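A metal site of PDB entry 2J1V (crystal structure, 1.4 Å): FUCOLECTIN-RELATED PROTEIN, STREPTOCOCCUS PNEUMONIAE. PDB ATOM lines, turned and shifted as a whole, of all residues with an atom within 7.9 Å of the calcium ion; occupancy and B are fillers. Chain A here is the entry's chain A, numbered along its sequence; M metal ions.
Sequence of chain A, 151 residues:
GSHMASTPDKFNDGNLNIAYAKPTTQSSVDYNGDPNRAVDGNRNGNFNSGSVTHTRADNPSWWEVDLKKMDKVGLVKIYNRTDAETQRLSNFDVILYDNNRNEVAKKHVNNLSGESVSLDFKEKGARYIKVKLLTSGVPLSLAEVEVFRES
The calcium ion is bound by O of Ala 143 (2.3 Å), O of Arg 37 (2.3 Å), O of Asn 42 (2.3 Å), OE1 of Glu 144 (2.4 Å), OD1 of Asp 40 (2.5 Å), O of Ser 51 (2.5 Å) and OG of Ser 51 (2.8 Å).
Of the 22 residues printed, 6 come within 4 Å of the calcium ion.
O of Glu 144 is in hydrogen-bond range of N of Tyr 79 (2.8 Å).
OE2 of Glu 144 lies within hydrogen-bond range of N of Gly 41 (2.8 Å).
The backbone carbonyl oxygen (O) of Asn 44 lies close to the side-chain hydroxyl (OG) of Ser 51, 2.8 Å away.
NE of Arg 37 lies close to O of Gly 50, 3.5 Å away.
The backbone NH (N) of Asn 44 lies within hydrogen-bond range of the side-chain amide oxygen (OD1) of Asn 42, at 3.1 Å.
N of Ala 143 sits at hydrogen-bond distance from O of Tyr 79, at 2.8 Å.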
ATOM      1  N   PRO A  35      21.973  29.699 -13.743  1.00  0.00           N
ATOM      2  CA  PRO A  35      23.185  30.503 -13.720  1.00  0.00           C
ATOM      3  C   PRO A  35      23.423  31.276 -12.436  1.00  0.00           C
ATOM      4  O   PRO A  35      24.619  31.570 -12.115  1.00  0.00           O
ATOM      5  CB  PRO A  35      23.021  31.429 -14.936  1.00  0.00           C
ATOM      6  CG  PRO A  35      21.519  31.475 -15.194  1.00  0.00           C
ATOM      7  CD  PRO A  35      21.053  30.080 -14.841  1.00  0.00           C
ATOM      8  N   ASN A  36      22.361  31.558 -11.678  1.00  0.00           N
ATOM      9  CA  ASN A  36      22.538  32.247 -10.385  1.00  0.00           C
ATOM     10  C   ASN A  36      23.312  31.443  -9.368  1.00  0.00           C
ATOM     11  O   ASN A  36      23.836  31.996  -8.406  1.00  0.00           O
ATOM     12  CB  ASN A  36      21.211  32.791  -9.847  1.00  0.00           C
ATOM     13  CG  ASN A  36      20.253  31.735  -9.277  1.00  0.00           C
ATOM     14  OD1 ASN A  36      19.367  32.087  -8.480  1.00  0.00           O
ATOM     15  ND2 ASN A  36      20.364  30.550  -9.680  1.00  0.00           N
ATOM     16  N   ARG A  37      23.499  30.130  -9.614  1.00  0.00           N
ATOM     17  CA  ARG A  37      24.253  29.342  -8.660  1.00  0.00           C
ATOM     18  C   ARG A  37      25.732  29.715  -8.629  1.00  0.00           C
ATOM     19  O   ARG A  37      26.436  29.434  -7.648  1.00  0.00           O
ATOM     20  CB  ARG A  37      24.044  27.848  -8.911  1.00  0.00           C
ATOM     21  CG  ARG A  37      22.655  27.400  -8.700  1.00  0.00           C
ATOM     22  CD  ARG A  37      22.354  25.962  -9.044  1.00  0.00           C
ATOM     23  NE  ARG A  37      20.911  25.690  -8.822  1.00  0.00           N
ATOM     24  CZ  ARG A  37      20.362  24.492  -8.736  1.00  0.00           C
ATOM     25  NH1 ARG A  37      19.035  24.354  -8.582  1.00  0.00           N
ATOM     26  NH2 ARG A  37      21.132  23.452  -8.803  1.00  0.00           N
ATOM     27  N   ALA A  38      26.238  30.421  -9.655  1.00  0.00           N
ATOM     28  CA  ALA A  38      27.627  30.837  -9.675  1.00  0.00           C
ATOM     29  C   ALA A  38      27.859  32.181  -8.982  1.00  0.00           C
ATOM     30  O   ALA A  38      28.980  32.645  -8.867  1.00  0.00           O
ATOM     31  CB  ALA A  38      28.179  30.869 -11.110  1.00  0.00           C
ATOM     32  N   VAL A  39      26.781  32.803  -8.494  1.00  0.00           N
ATOM     33  CA  VAL A  39      26.903  34.064  -7.740  1.00  0.00           C
ATOM     34  C   VAL A  39      26.150  34.028  -6.395  1.00  0.00           C
ATOM     35  O   VAL A  39      25.713  35.057  -5.885  1.00  0.00           O
ATOM     36  CB  VAL A  39      26.492  35.326  -8.602  1.00  0.00           C
ATOM     37  CG1 VAL A  39      27.424  35.445  -9.785  1.00  0.00           C
ATOM     38  CG2 VAL A  39      25.035  35.287  -9.030  1.00  0.00           C
ATOM     39  N   ASP A  40      26.015  32.821  -5.864  1.00  0.00           N
ATOM     40  CA  ASP A  40      25.221  32.625  -4.643  1.00  0.00           C
ATOM     41  C   ASP A  40      26.083  32.663  -3.382  1.00  0.00           C
ATOM     42  O   ASP A  40      25.543  32.498  -2.275  1.00  0.00           O
ATOM     43  CB  ASP A  40      24.371  31.336  -4.726  1.00  0.00           C
ATOM     44  CG  ASP A  40      25.169  30.068  -4.739  1.00  0.00           C
ATOM     45  OD1 ASP A  40      26.410  30.094  -4.728  1.00  0.00           O
ATOM     46  OD2 ASP A  40      24.541  28.963  -4.740  1.00  0.00           O
ATOM     47  N   GLY A  41      27.357  32.996  -3.514  1.00  0.00           N
ATOM     48  CA  GLY A  41      28.266  33.117  -2.374  1.00  0.00           C
ATOM     49  C   GLY A  41      28.778  31.795  -1.844  1.00  0.00           C
ATOM     50  O   GLY A  41      29.475  31.793  -0.811  1.00  0.00           O
ATOM     51  N   ASN A  42      28.495  30.718  -2.542  1.00  0.00           N
ATOM     52  CA  ASN A  42      28.817  29.352  -2.133  1.00  0.00           C
ATOM     53  C   ASN A  42      29.812  28.737  -3.109  1.00  0.00           C
ATOM     54  O   ASN A  42      29.440  28.483  -4.268  1.00  0.00           O
ATOM     55  CB  ASN A  42      27.556  28.503  -1.993  1.00  0.00           C
ATOM     56  CG  ASN A  42      27.846  27.112  -1.448  1.00  0.00           C
ATOM     57  OD1 ASN A  42      28.973  26.807  -1.105  1.00  0.00           O
ATOM     58  ND2 ASN A  42      26.804  26.331  -1.293  1.00  0.00           N
ATOM     59  N   ARG A  43      31.045  28.497  -2.676  1.00  0.00           N
ATOM     60  CA  ARG A  43      32.075  27.944  -3.563  1.00  0.00           C
ATOM     61  C   ARG A  43      32.042  26.416  -3.719  1.00  0.00           C
ATOM     62  O   ARG A  43      32.828  25.849  -4.470  1.00  0.00           O
ATOM     63  CB  ARG A  43      33.451  28.330  -3.080  1.00  0.00           C
ATOM     64  CG  ARG A  43      33.752  29.819  -3.058  1.00  0.00           C
ATOM     65  CD  ARG A  43      35.102  30.116  -2.392  1.00  0.00           C
ATOM     66  NE  ARG A  43      35.448  31.534  -2.448  1.00  0.00           N
ATOM     67  CZ  ARG A  43      36.528  32.035  -1.872  1.00  0.00           C
ATOM     68  NH1 ARG A  43      36.786  33.344  -1.966  1.00  0.00           N
ATOM     69  NH2 ARG A  43      37.397  31.244  -1.225  1.00  0.00           N
ATOM     70  N   ASN A  44      31.145  25.747  -2.991  1.00  0.00           N
ATOM     71  CA  ASN A  44      31.022  24.282  -3.036  1.00  0.00           C
ATOM     72  C   ASN A  44      30.872  23.831  -4.475  1.00  0.00           C
ATOM     73  O   ASN A  44      29.923  24.219  -5.153  1.00  0.00           O
ATOM     74  CB  ASN A  44      29.808  23.848  -2.182  1.00  0.00           C
ATOM     75  CG  ASN A  44      29.749  22.348  -1.916  1.00  0.00           C
ATOM     76  OD1 ASN A  44      29.131  21.905  -0.904  1.00  0.00           O
ATOM     77  ND2 ASN A  44      30.350  21.573  -2.744  1.00  0.00           N
ATOM     78  N   GLY A  45      31.827  23.029  -4.949  1.00  0.00           N
ATOM     79  CA  GLY A  45      31.792  22.531  -6.313  1.00  0.00           C
ATOM     80  C   GLY A  45      31.180  21.177  -6.546  1.00  0.00           C
ATOM     81  O   GLY A  45      31.237  20.635  -7.655  1.00  0.00           O
ATOM     82  N   SER A  49      25.162  19.269  -4.470  1.00  0.00           N
ATOM     83  CA  SER A  49      24.915  20.151  -3.332  1.00  0.00           C
ATOM     84  C   SER A  49      24.127  21.400  -3.694  1.00  0.00           C
ATOM     85  O   SER A  49      23.665  22.108  -2.828  1.00  0.00           O
ATOM     86  CB  SER A  49      26.214  20.534  -2.669  1.00  0.00           C
ATOM     87  OG  SER A  49      26.709  21.765  -3.208  1.00  0.00           O
ATOM     88  N   GLY A  50      23.936  21.699  -4.983  1.00  0.00           N
ATOM     89  CA  GLY A  50      23.075  22.786  -5.382  1.00  0.00           C
ATOM     90  C   GLY A  50      23.715  24.103  -5.733  1.00  0.00           C
ATOM     91  O   GLY A  50      23.004  25.032  -6.098  1.00  0.00           O
ATOM     92  N   SER A  51      25.038  24.204  -5.606  1.00  0.00           N
ATOM     93  CA  SER A  51      25.724  25.486  -5.800  1.00  0.00           C
ATOM     94  C   SER A  51      26.487  25.651  -7.117  1.00  0.00           C
ATOM     95  O   SER A  51      27.225  26.610  -7.218  1.00  0.00           O
ATOM     96  CB  SER A  51      26.672  25.680  -4.600  1.00  0.00           C
ATOM     97  OG  SER A  51      28.021  26.193  -4.834  1.00  0.00           O
ATOM     98  N   VAL A  52      26.241  24.767  -8.074  1.00  0.00           N
ATOM     99  CA  VAL A  52      26.996  24.676  -9.314  1.00  0.00           C
ATOM    100  C   VAL A  52      26.039  24.794 -10.501  1.00  0.00           C
ATOM    101  O   VAL A  52      24.992  24.148 -10.562  1.00  0.00           O
ATOM    102  CB  VAL A  52      27.775  23.334  -9.393  1.00  0.00           C
ATOM    103  CG1 VAL A  52      28.691  23.208 -10.651  1.00  0.00           C
ATOM    104  CG2 VAL A  52      28.622  23.113  -8.156  1.00  0.00           C
ATOM    105  N   THR A  53      26.439  25.628 -11.466  1.00  0.00           N
ATOM    106  CA  THR A  53      25.648  25.813 -12.696  1.00  0.00           C
ATOM    107  C   THR A  53      25.793  24.627 -13.630  1.00  0.00           C
ATOM    108  O   THR A  53      26.683  23.792 -13.457  1.00  0.00           O
ATOM    109  CB  THR A  53      26.064  27.085 -13.436  1.00  0.00           C
ATOM    110  OG1 THR A  53      27.358  26.878 -13.985  1.00  0.00           O
ATOM    111  CG2 THR A  53      26.119  28.322 -12.511  1.00  0.00           C
ATOM    112  N   TYR A  79      35.702  29.286  -9.930  1.00  0.00           N
ATOM    113  CA  TYR A  79      35.748  28.054  -9.120  1.00  0.00           C
ATOM    114  C   TYR A  79      35.039  26.955  -9.912  1.00  0.00           C
ATOM    115  O   TYR A  79      33.886  27.117 -10.327  1.00  0.00           O
ATOM    116  CB  TYR A  79      35.083  28.290  -7.760  1.00  0.00           C
ATOM    117  CG  TYR A  79      35.827  29.269  -6.877  1.00  0.00           C
ATOM    118  CD1 TYR A  79      36.746  28.848  -5.943  1.00  0.00           C
ATOM    119  CD2 TYR A  79      35.602  30.640  -7.029  1.00  0.00           C
ATOM    120  CE1 TYR A  79      37.465  29.769  -5.218  1.00  0.00           C
ATOM    121  CE2 TYR A  79      36.312  31.572  -6.305  1.00  0.00           C
ATOM    122  CZ  TYR A  79      37.202  31.125  -5.397  1.00  0.00           C
ATOM    123  OH  TYR A  79      37.853  32.092  -4.660  1.00  0.00           O
ATOM    124  N   LEU A 142      29.954  25.878 -13.428  1.00  0.00           N
ATOM    125  CA  LEU A 142      30.791  26.753 -12.638  1.00  0.00           C
ATOM    126  C   LEU A 142      30.247  26.700 -11.203  1.00  0.00           C
ATOM    127  O   LEU A 142      29.026  26.879 -10.979  1.00  0.00           O
ATOM    128  CB  LEU A 142      30.687  28.195 -13.163  1.00  0.00           C
ATOM    129  CG  LEU A 142      31.206  28.410 -14.585  1.00  0.00           C
ATOM    130  CD1 LEU A 142      30.845  29.770 -15.152  1.00  0.00           C
ATOM    131  CD2 LEU A 142      32.716  28.102 -14.651  1.00  0.00           C
ATOM    132  N   ALA A 143      31.129  26.452 -10.235  1.00  0.00           N
ATOM    133  CA  ALA A 143      30.730  26.486  -8.825  1.00  0.00           C
ATOM    134  C   ALA A 143      30.505  27.920  -8.357  1.00  0.00           C
ATOM    135  O   ALA A 143      29.590  28.186  -7.568  1.00  0.00           O
ATOM    136  CB  ALA A 143      31.784  25.824  -7.953  1.00  0.00           C
ATOM    137  N   GLU A 144      31.369  28.847  -8.794  1.00  0.00           N
ATOM    138  CA  GLU A 144      31.250  30.224  -8.394  1.00  0.00           C
ATOM    139  C   GLU A 144      32.167  31.071  -9.273  1.00  0.00           C
ATOM    140  O   GLU A 144      33.229  30.616  -9.664  1.00  0.00           O
ATOM    141  CB  GLU A 144      31.650  30.406  -6.921  1.00  0.00           C
ATOM    142  CG  GLU A 144      31.208  31.721  -6.297  1.00  0.00           C
ATOM    143  CD  GLU A 144      29.723  31.851  -5.973  1.00  0.00           C
ATOM    144  OE1 GLU A 144      28.944  30.883  -6.162  1.00  0.00           O
ATOM    145  OE2 GLU A 144      29.319  32.963  -5.555  1.00  0.00           O
ATOM    146  N   VAL A 145      31.741  32.299  -9.551  1.00  0.00           N
ATOM    147  CA  VAL A 145      32.573  33.312 -10.202  1.00  0.00           C
ATOM    148  C   VAL A 145      32.536  34.562  -9.331  1.00  0.00           C
ATOM    149  O   VAL A 145      31.489  35.117  -9.114  1.00  0.00           O
ATOM    150  CB  VAL A 145      32.071  33.642 -11.637  1.00  0.00           C
ATOM    151  CG1 VAL A 145      32.908  34.743 -12.252  1.00  0.00           C
ATOM    152  CG2 VAL A 145      32.104  32.424 -12.528  1.00  0.00           C
ATOM    153  N   GLU A 146      33.688  34.927  -8.791  1.00  0.00           N
ATOM    154  CA  GLU A 146      33.833  36.078  -7.927  1.00  0.00           C
ATOM    155  C   GLU A 146      34.590  37.148  -8.718  1.00  0.00           C
ATOM    156  O   GLU A 146      35.568  36.840  -9.408  1.00  0.00           O
ATOM    157  CB  GLU A 146      34.581  35.653  -6.644  1.00  0.00           C
ATOM    158  CG  GLU A 146      33.776  34.647  -5.827  1.00  0.00           C
ATOM    159  CD  GLU A 146      34.464  34.180  -4.584  1.00  0.00           C
ATOM    160  OE1 GLU A 146      35.686  34.530  -4.409  1.00  0.00           O
ATOM    161  OE2 GLU A 146      33.797  33.396  -3.848  1.00  0.00           O
HETATM  162 CA    CA M   1      27.937  28.692  -6.046  1.00  0.00          CA
